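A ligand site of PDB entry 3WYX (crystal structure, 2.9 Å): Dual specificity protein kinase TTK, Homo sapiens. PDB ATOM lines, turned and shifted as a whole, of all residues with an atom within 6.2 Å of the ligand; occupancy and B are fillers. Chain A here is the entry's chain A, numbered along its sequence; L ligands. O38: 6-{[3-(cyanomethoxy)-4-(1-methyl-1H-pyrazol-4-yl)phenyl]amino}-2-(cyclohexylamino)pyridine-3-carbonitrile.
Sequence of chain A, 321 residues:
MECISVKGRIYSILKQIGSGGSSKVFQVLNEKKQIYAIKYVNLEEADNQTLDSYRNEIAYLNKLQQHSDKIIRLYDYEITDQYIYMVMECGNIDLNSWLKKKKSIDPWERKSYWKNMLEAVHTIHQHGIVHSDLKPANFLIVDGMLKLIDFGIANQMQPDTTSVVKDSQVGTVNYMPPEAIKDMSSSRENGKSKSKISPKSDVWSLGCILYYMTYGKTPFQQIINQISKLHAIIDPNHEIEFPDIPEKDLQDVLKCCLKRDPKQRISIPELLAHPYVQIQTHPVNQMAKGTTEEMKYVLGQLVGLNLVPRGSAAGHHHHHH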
ATOM      1  N   LYS A  15      24.982 -23.539   8.751  1.00  0.00           N
ATOM      2  CA  LYS A  15      25.524 -23.419  10.086  1.00  0.00           C
ATOM      3  C   LYS A  15      24.655 -24.249  11.054  1.00  0.00           C
ATOM      4  O   LYS A  15      23.782 -25.005  10.632  1.00  0.00           O
ATOM      5  CB  LYS A  15      25.591 -21.939  10.495  1.00  0.00           C
ATOM      6  CG  LYS A  15      24.246 -21.217  10.515  1.00  0.00           C
ATOM      7  CD  LYS A  15      24.253 -19.965  11.384  1.00  0.00           C
ATOM      8  CE  LYS A  15      22.963 -19.176  11.251  1.00  0.00           C
ATOM      9  N   ILE A  17      22.304 -23.842  14.562  1.00  0.00           N
ATOM     10  CA  ILE A  17      21.546 -22.882  15.356  1.00  0.00           C
ATOM     11  C   ILE A  17      21.547 -23.292  16.829  1.00  0.00           C
ATOM     12  O   ILE A  17      21.549 -22.426  17.717  1.00  0.00           O
ATOM     13  CB  ILE A  17      20.075 -22.793  14.855  1.00  0.00           C
ATOM     14  CG1 ILE A  17      20.013 -22.433  13.365  1.00  0.00           C
ATOM     15  CG2 ILE A  17      19.276 -21.789  15.682  1.00  0.00           C
ATOM     16  CD1 ILE A  17      18.672 -22.688  12.703  1.00  0.00           C
ATOM     17  N   GLY A  18      21.554 -24.607  17.081  1.00  0.00           N
ATOM     18  CA  GLY A  18      21.368 -25.142  18.436  1.00  0.00           C
ATOM     19  C   GLY A  18      21.880 -26.568  18.610  1.00  0.00           C
ATOM     20  O   GLY A  18      22.217 -27.234  17.636  1.00  0.00           O
ATOM     21  N   SER A  19      21.952 -27.009  19.869  1.00  0.00           N
ATOM     22  CA  SER A  19      22.433 -28.345  20.211  1.00  0.00           C
ATOM     23  C   SER A  19      21.959 -28.735  21.608  1.00  0.00           C
ATOM     24  O   SER A  19      22.215 -28.022  22.587  1.00  0.00           O
ATOM     25  CB  SER A  19      23.962 -28.414  20.181  1.00  0.00           C
ATOM     26  OG  SER A  19      24.557 -27.748  21.285  1.00  0.00           O
ATOM     27  N   VAL A  25      20.175 -28.579  15.887  1.00  0.00           N
ATOM     28  CA  VAL A  25      19.373 -27.794  14.934  1.00  0.00           C
ATOM     29  C   VAL A  25      20.262 -27.017  13.938  1.00  0.00           C
ATOM     30  O   VAL A  25      21.207 -26.334  14.324  1.00  0.00           O
ATOM     31  CB  VAL A  25      18.430 -26.793  15.653  1.00  0.00           C
ATOM     32  CG1 VAL A  25      17.560 -26.046  14.634  1.00  0.00           C
ATOM     33  CG2 VAL A  25      17.550 -27.511  16.665  1.00  0.00           C
ATOM     34  N   GLN A  27      20.636 -24.562  10.172  1.00  0.00           N
ATOM     35  CA  GLN A  27      20.109 -23.760   9.091  1.00  0.00           C
ATOM     36  C   GLN A  27      20.564 -24.435   7.807  1.00  0.00           C
ATOM     37  O   GLN A  27      21.749 -24.693   7.643  1.00  0.00           O
ATOM     38  CB  GLN A  27      20.637 -22.343   9.186  1.00  0.00           C
ATOM     39  CG  GLN A  27      20.054 -21.374   8.167  1.00  0.00           C
ATOM     40  CD  GLN A  27      20.742 -20.027   8.196  1.00  0.00           C
ATOM     41  OE1 GLN A  27      20.086 -19.000   8.346  1.00  0.00           O
ATOM     42  NE2 GLN A  27      22.072 -20.029   8.094  1.00  0.00           N
ATOM     43  N   ILE A  35      15.633 -21.682   2.331  1.00  0.00           N
ATOM     44  CA  ILE A  35      16.145 -21.816   3.694  1.00  0.00           C
ATOM     45  C   ILE A  35      15.174 -22.607   4.563  1.00  0.00           C
ATOM     46  O   ILE A  35      13.960 -22.425   4.473  1.00  0.00           O
ATOM     47  CB  ILE A  35      16.435 -20.415   4.290  1.00  0.00           C
ATOM     48  CG1 ILE A  35      17.428 -20.498   5.433  1.00  0.00           C
ATOM     49  CG2 ILE A  35      15.169 -19.705   4.769  1.00  0.00           C
ATOM     50  CD1 ILE A  35      17.903 -19.133   5.868  1.00  0.00           C
ATOM     51  N   ALA A  37      15.000 -25.170   8.567  1.00  0.00           N
ATOM     52  CA  ALA A  37      15.665 -25.605   9.790  1.00  0.00           C
ATOM     53  C   ALA A  37      15.434 -27.097   9.977  1.00  0.00           C
ATOM     54  O   ALA A  37      14.305 -27.562   9.933  1.00  0.00           O
ATOM     55  CB  ALA A  37      15.147 -24.829  10.991  1.00  0.00           C
ATOM     56  N   ILE A  38      16.518 -27.840  10.193  1.00  0.00           N
ATOM     57  CA  ILE A  38      16.429 -29.285  10.387  1.00  0.00           C
ATOM     58  C   ILE A  38      16.830 -29.659  11.798  1.00  0.00           C
ATOM     59  O   ILE A  38      17.969 -29.430  12.197  1.00  0.00           O
ATOM     60  CB  ILE A  38      17.274 -30.074   9.349  1.00  0.00           C
ATOM     61  CG1 ILE A  38      16.602 -29.963   7.975  1.00  0.00           C
ATOM     62  CG2 ILE A  38      17.393 -31.542   9.764  1.00  0.00           C
ATOM     63  CD1 ILE A  38      17.259 -30.734   6.845  1.00  0.00           C
ATOM     64  N   LYS A  39      15.882 -30.224  12.549  1.00  0.00           N
ATOM     65  CA  LYS A  39      16.198 -30.773  13.854  1.00  0.00           C
ATOM     66  C   LYS A  39      16.635 -32.217  13.651  1.00  0.00           C
ATOM     67  O   LYS A  39      15.869 -33.037  13.176  1.00  0.00           O
ATOM     68  CB  LYS A  39      14.989 -30.725  14.782  1.00  0.00           C
ATOM     69  CG  LYS A  39      15.411 -30.711  16.239  1.00  0.00           C
ATOM     70  CD  LYS A  39      14.496 -31.513  17.145  1.00  0.00           C
ATOM     71  CE  LYS A  39      13.377 -30.678  17.762  1.00  0.00           C
ATOM     72  NZ  LYS A  39      12.905 -31.291  19.050  1.00  0.00           N
ATOM     73  N   ILE A  72       4.843 -23.737  14.745  1.00  0.00           N
ATOM     74  CA  ILE A  72       5.854 -23.873  13.710  1.00  0.00           C
ATOM     75  C   ILE A  72       5.445 -24.924  12.670  1.00  0.00           C
ATOM     76  O   ILE A  72       4.749 -25.876  12.980  1.00  0.00           O
ATOM     77  CB  ILE A  72       7.228 -24.214  14.329  1.00  0.00           C
ATOM     78  CG1 ILE A  72       8.336 -24.041  13.276  1.00  0.00           C
ATOM     79  CG2 ILE A  72       7.201 -25.609  14.954  1.00  0.00           C
ATOM     80  CD1 ILE A  72       9.729 -24.062  13.831  1.00  0.00           C
ATOM     81  N   MET A  88      11.731 -28.069   9.172  1.00  0.00           N
ATOM     82  CA  MET A  88      10.811 -27.069   9.692  1.00  0.00           C
ATOM     83  C   MET A  88      11.100 -25.674   9.122  1.00  0.00           C
ATOM     84  O   MET A  88      12.064 -25.472   8.380  1.00  0.00           O
ATOM     85  CB  MET A  88      10.938 -27.020  11.226  1.00  0.00           C
ATOM     86  CG  MET A  88      10.914 -28.386  11.905  1.00  0.00           C
ATOM     87  SD  MET A  88      11.571 -28.371  13.581  1.00  0.00           S
ATOM     88  CE  MET A  88      10.203 -27.681  14.495  1.00  0.00           C
ATOM     89  N   GLU A  89      10.247 -24.712   9.483  1.00  0.00           N
ATOM     90  CA  GLU A  89      10.501 -23.309   9.198  1.00  0.00           C
ATOM     91  C   GLU A  89      11.796 -22.908   9.856  1.00  0.00           C
ATOM     92  O   GLU A  89      12.083 -23.307  10.987  1.00  0.00           O
ATOM     93  CB  GLU A  89       9.420 -22.420   9.796  1.00  0.00           C
ATOM     94  CG  GLU A  89       8.127 -22.323   9.012  1.00  0.00           C
ATOM     95  CD  GLU A  89       7.116 -21.421   9.707  1.00  0.00           C
ATOM     96  OE1 GLU A  89       6.219 -21.932  10.403  1.00  0.00           O
ATOM     97  OE2 GLU A  89       7.251 -20.186   9.587  1.00  0.00           O
ATOM     98  N   CYS A  90      12.576 -22.074   9.163  1.00  0.00           N
ATOM     99  CA  CYS A  90      13.800 -21.553   9.726  1.00  0.00           C
ATOM    100  C   CYS A  90      13.490 -20.318  10.550  1.00  0.00           C
ATOM    101  O   CYS A  90      14.065 -20.141  11.622  1.00  0.00           O
ATOM    102  CB  CYS A  90      14.796 -21.217   8.626  1.00  0.00           C
ATOM    103  SG  CYS A  90      16.435 -20.929   9.306  1.00  0.00           S
ATOM    104  N   GLY A  91      12.586 -19.476  10.049  1.00  0.00           N
ATOM    105  CA  GLY A  91      12.258 -18.225  10.752  1.00  0.00           C
ATOM    106  C   GLY A  91      13.415 -17.229  10.784  1.00  0.00           C
ATOM    107  O   GLY A  91      14.323 -17.315   9.958  1.00  0.00           O
ATOM    108  N   ASN A  92      13.375 -16.287  11.723  1.00  0.00           N
ATOM    109  CA  ASN A  92      14.404 -15.241  11.841  1.00  0.00           C
ATOM    110  C   ASN A  92      15.212 -15.396  13.109  1.00  0.00           C
ATOM    111  O   ASN A  92      16.434 -15.338  13.089  1.00  0.00           O
ATOM    112  CB  ASN A  92      13.790 -13.839  11.830  1.00  0.00           C
ATOM    113  CG  ASN A  92      12.902 -13.586  10.637  1.00  0.00           C
ATOM    114  OD1 ASN A  92      12.748 -14.414   9.739  1.00  0.00           O
ATOM    115  ND2 ASN A  92      12.287 -12.408  10.623  1.00  0.00           N
ATOM    116  N   ILE A  93      14.530 -15.568  14.232  1.00  0.00           N
ATOM    117  CA  ILE A  93      15.216 -15.684  15.506  1.00  0.00           C
ATOM    118  C   ILE A  93      14.266 -16.100  16.619  1.00  0.00           C
ATOM    119  O   ILE A  93      13.093 -15.759  16.596  1.00  0.00           O
ATOM    120  CB  ILE A  93      15.837 -14.332  15.896  1.00  0.00           C
ATOM    121  CG1 ILE A  93      16.682 -14.479  17.159  1.00  0.00           C
ATOM    122  CG2 ILE A  93      14.750 -13.290  16.107  1.00  0.00           C
ATOM    123  CD1 ILE A  93      17.568 -13.281  17.398  1.00  0.00           C
ATOM    124  N   ASP A  94      14.802 -16.818  17.605  1.00  0.00           N
ATOM    125  CA  ASP A  94      14.030 -17.211  18.794  1.00  0.00           C
ATOM    126  C   ASP A  94      13.705 -16.013  19.690  1.00  0.00           C
ATOM    127  O   ASP A  94      14.422 -15.030  19.692  1.00  0.00           O
ATOM    128  CB  ASP A  94      14.743 -18.313  19.579  1.00  0.00           C
ATOM    129  CG  ASP A  94      15.992 -17.827  20.275  1.00  0.00           C
ATOM    130  OD1 ASP A  94      16.973 -17.520  19.570  1.00  0.00           O
ATOM    131  OD2 ASP A  94      16.009 -17.779  21.532  1.00  0.00           O
ATOM    132  N   SER A  97      16.535 -14.849  22.445  1.00  0.00           N
ATOM    133  CA  SER A  97      17.663 -14.077  21.938  1.00  0.00           C
ATOM    134  C   SER A  97      17.256 -12.661  21.517  1.00  0.00           C
ATOM    135  O   SER A  97      17.975 -11.693  21.767  1.00  0.00           O
ATOM    136  CB  SER A  97      18.343 -14.822  20.784  1.00  0.00           C
ATOM    137  OG  SER A  97      18.796 -16.104  21.211  1.00  0.00           O
ATOM    138  N   ALA A 137      12.583 -19.011  24.590  1.00  0.00           N
ATOM    139  CA  ALA A 137      13.292 -19.866  23.637  1.00  0.00           C
ATOM    140  C   ALA A 137      12.386 -20.864  22.931  1.00  0.00           C
ATOM    141  O   ALA A 137      12.780 -21.442  21.914  1.00  0.00           O
ATOM    142  CB  ALA A 137      14.431 -20.601  24.327  1.00  0.00           C
ATOM    143  N   ASN A 138      11.170 -21.066  23.453  1.00  0.00           N
ATOM    144  CA  ASN A 138      10.169 -21.916  22.806  1.00  0.00           C
ATOM    145  C   ASN A 138       9.399 -21.218  21.671  1.00  0.00           C
ATOM    146  O   ASN A 138       8.601 -21.873  20.981  1.00  0.00           O
ATOM    147  CB  ASN A 138       9.159 -22.463  23.820  1.00  0.00           C
ATOM    148  CG  ASN A 138       9.752 -23.535  24.704  1.00  0.00           C
ATOM    149  OD1 ASN A 138       9.819 -23.402  25.925  1.00  0.00           O
ATOM    150  ND2 ASN A 138      10.172 -24.604  24.087  1.00  0.00           N
ATOM    151  N   LEU A 140       9.393 -18.726  18.099  1.00  0.00           N
ATOM    152  CA  LEU A 140      10.173 -18.355  16.936  1.00  0.00           C
ATOM    153  C   LEU A 140       9.506 -17.181  16.213  1.00  0.00           C
ATOM    154  O   LEU A 140       8.317 -17.231  15.907  1.00  0.00           O
ATOM    155  CB  LEU A 140      10.277 -19.554  15.979  1.00  0.00           C
ATOM    156  CG  LEU A 140      11.105 -19.371  14.700  1.00  0.00           C
ATOM    157  CD1 LEU A 140      12.567 -19.146  15.057  1.00  0.00           C
ATOM    158  CD2 LEU A 140      10.951 -20.565  13.761  1.00  0.00           C
ATOM    159  N   ILE A 149       7.451 -23.503  18.914  1.00  0.00           N
ATOM    160  CA  ILE A 149       8.417 -24.415  18.308  1.00  0.00           C
ATOM    161  C   ILE A 149       8.156 -25.833  18.797  1.00  0.00           C
ATOM    162  O   ILE A 149       8.101 -26.758  17.991  1.00  0.00           O
ATOM    163  CB  ILE A 149       9.872 -24.015  18.673  1.00  0.00           C
ATOM    164  CG1 ILE A 149      10.170 -22.582  18.216  1.00  0.00           C
ATOM    165  CG2 ILE A 149      10.873 -24.972  18.027  1.00  0.00           C
ATOM    166  CD1 ILE A 149      11.438 -22.005  18.782  1.00  0.00           C
ATOM    167  N   ASP A 150       8.014 -25.994  20.119  1.00  0.00           N
ATOM    168  CA  ASP A 150       7.771 -27.315  20.722  1.00  0.00           C
ATOM    169  C   ASP A 150       6.737 -27.280  21.842  1.00  0.00           C
ATOM    170  O   ASP A 150       6.211 -26.219  22.167  1.00  0.00           O
ATOM    171  CB  ASP A 150       9.081 -27.889  21.235  1.00  0.00           C
ATOM    172  CG  ASP A 150       9.727 -27.034  22.274  1.00  0.00           C
ATOM    173  OD1 ASP A 150       9.224 -26.996  23.419  1.00  0.00           O
ATOM    174  OD2 ASP A 150      10.754 -26.387  21.945  1.00  0.00           O
ATOM    175  N   MET A 157      16.262 -27.349  24.690  1.00  0.00           N
ATOM    176  CA  MET A 157      17.445 -27.041  23.866  1.00  0.00           C
ATOM    177  C   MET A 157      17.893 -25.575  23.970  1.00  0.00           C
ATOM    178  O   MET A 157      17.039 -24.689  24.106  1.00  0.00           O
ATOM    179  CB  MET A 157      17.134 -27.380  22.398  1.00  0.00           C
ATOM    180  CG  MET A 157      18.272 -27.993  21.591  1.00  0.00           C
ATOM    181  SD  MET A 157      17.644 -28.741  20.067  1.00  0.00           S
ATOM    182  CE  MET A 157      19.120 -29.447  19.385  1.00  0.00           C
ATOM    183  N   GLN A 158      19.204 -25.340  23.871  1.00  0.00           N
ATOM    184  CA  GLN A 158      19.816 -24.002  24.052  1.00  0.00           C
ATOM    185  C   GLN A 158      20.715 -23.658  22.855  1.00  0.00           C
ATOM    186  O   GLN A 158      21.246 -24.557  22.209  1.00  0.00           O
ATOM    187  CB  GLN A 158      20.638 -23.963  25.346  1.00  0.00           C
ATOM    188  N   PRO A 159      20.907 -22.352  22.554  1.00  0.00           N
ATOM    189  CA  PRO A 159      21.625 -21.982  21.324  1.00  0.00           C
ATOM    190  C   PRO A 159      23.139 -22.118  21.427  1.00  0.00           C
ATOM    191  O   PRO A 159      23.802 -22.406  20.419  1.00  0.00           O
ATOM    192  CB  PRO A 159      21.227 -20.509  21.125  1.00  0.00           C
ATOM    193  CG  PRO A 159      20.989 -19.995  22.504  1.00  0.00           C
ATOM    194  CD  PRO A 159      20.526 -21.159  23.340  1.00  0.00           C
HETATM  195  N6  O38 L   1      17.010 -18.078   9.839  1.00  0.00           N
HETATM  196  C23 O38 L   1      17.695 -18.078  10.772  1.00  0.00           C
HETATM  197  C22 O38 L   1      18.576 -18.054  11.959  1.00  0.00           C
HETATM  198  O   O38 L   1      17.860 -17.500  13.064  1.00  0.00           O
HETATM  199  C21 O38 L   1      17.378 -18.372  14.017  1.00  0.00           C
HETATM  200  C4  O38 L   1      17.808 -18.362  15.339  1.00  0.00           C
HETATM  201  C2  O38 L   1      18.747 -17.418  15.775  1.00  0.00           C
HETATM  202  C1  O38 L   1      19.236 -17.310  17.076  1.00  0.00           C
HETATM  203  C3  O38 L   1      19.364 -16.411  15.018  1.00  0.00           C
HETATM  204  N1  O38 L   1      20.197 -15.705  15.810  1.00  0.00           N
HETATM  205  N   O38 L   1      20.099 -16.288  17.084  1.00  0.00           N
HETATM  206  C   O38 L   1      20.956 -15.678  18.142  1.00  0.00           C
HETATM  207  C20 O38 L   1      16.444 -19.315  13.589  1.00  0.00           C
HETATM  208  C7  O38 L   1      15.913 -20.255  14.430  1.00  0.00           C
HETATM  209  C6  O38 L   1      16.332 -20.240  15.759  1.00  0.00           C
HETATM  210  C5  O38 L   1      17.252 -19.306  16.199  1.00  0.00           C
HETATM  211  N2  O38 L   1      15.049 -21.148  13.868  1.00  0.00           N
HETATM  212  C8  O38 L   1      14.665 -22.342  14.418  1.00  0.00           C
HETATM  213  N5  O38 L   1      15.057 -22.723  15.657  1.00  0.00           N
HETATM  214  C13 O38 L   1      14.673 -23.882  16.196  1.00  0.00           C
HETATM  215  C11 O38 L   1      13.841 -24.753  15.475  1.00  0.00           C
HETATM  216  C12 O38 L   1      13.467 -25.890  15.962  1.00  0.00           C
HETATM  217  N3  O38 L   1      13.225 -26.945  16.401  1.00  0.00           N
HETATM  218  C10 O38 L   1      13.414 -24.409  14.209  1.00  0.00           C
HETATM  219  C9  O38 L   1      13.831 -23.189  13.679  1.00  0.00           C
HETATM  220  N4  O38 L   1      15.116 -24.204  17.431  1.00  0.00           N
HETATM  221  C14 O38 L   1      16.086 -23.414  18.183  1.00  0.00           C
HETATM  222  C19 O38 L   1      17.218 -24.328  18.642  1.00  0.00           C
HETATM  223  C18 O38 L   1      18.093 -23.749  19.747  1.00  0.00           C
HETATM  224  C17 O38 L   1      17.279 -23.145  20.876  1.00  0.00           C
HETATM  225  C16 O38 L   1      16.313 -22.085  20.352  1.00  0.00           C
HETATM  226  C15 O38 L   1      15.368 -22.723  19.357  1.00  0.00           C
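A nitrogen (N2) of the ligand lies within hydrogen-bond range of the backbone carbonyl oxygen (O) of Cys 90 (2.7 Å).
The side-chain sulfur of Cys 90 is in hydrogen-bond range of a nitrogen (N6) of the ligand.
The backbone carbonyl oxygen (O) of Asn 92 sits close to an oxygen (O) of the ligand (2.6 Å).
The backbone NH (N) of Ile 149 is in hydrogen-bond range of the backbone carbonyl oxygen (O) of Asn 138, 2.9 Å away.
The backbone NH (N) of Met 88 sits at hydrogen-bond distance from the backbone carbonyl oxygen (O) of Ala 37, at 2.7 Å.
N of Gln 27 lies within hydrogen-bond range of O of Lys 15.
The backbone carbonyl oxygen (O) of Gln 158 is in hydrogen-bond range of the backbone NH (N) of Ser 19.
N of Val 25 is in hydrogen-bond range of O of Gly 18.
OG of Ser 97 is in hydrogen-bond range of OD1 of Asp 94, 2.8 Å away.
The backbone NH (N) of Ile 17 sits at hydrogen-bond distance from the backbone carbonyl oxygen (O) of Val 25.
The side-chain sulfur (SD) of Met 88 sits close to a nitrogen (N3) of the ligand.
The backbone carbonyl oxygen of Gly 91 sits close to a nitrogen (N6) of the ligand, 2.8 Å away.
Residues that only touch the ligand: Glu 89, Ile 17, Asp 94, Leu 140, Ala 37, Ile 149, Gln 27, Met 157, Ile 72, Ile 93, Val 25, Ser 97, Gly 18, Ala 137, Lys 39 and Gln 158.
Hydrophobic or aromatic side chains within 4 Å of the ligand: Ile 17, Val 25, Ala 37, Ile 72, Met 88, Ile 93, Leu 140 and Ile 149.
Within 4 Å of the ligand: Ile 17, Gly 18, Val 25, Gln 27, Ala 37, Lys 39, Ile 72, Met 88, Glu 89, Cys 90, Gly 91, Asn 92, Ile 93, Asp 94, Ser 97, Ala 137, Leu 140, Ile 149, Met 157 and Gln 158.
The nearest printed residue that does not touch the ligand is Pro 159 (4.1 Å).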
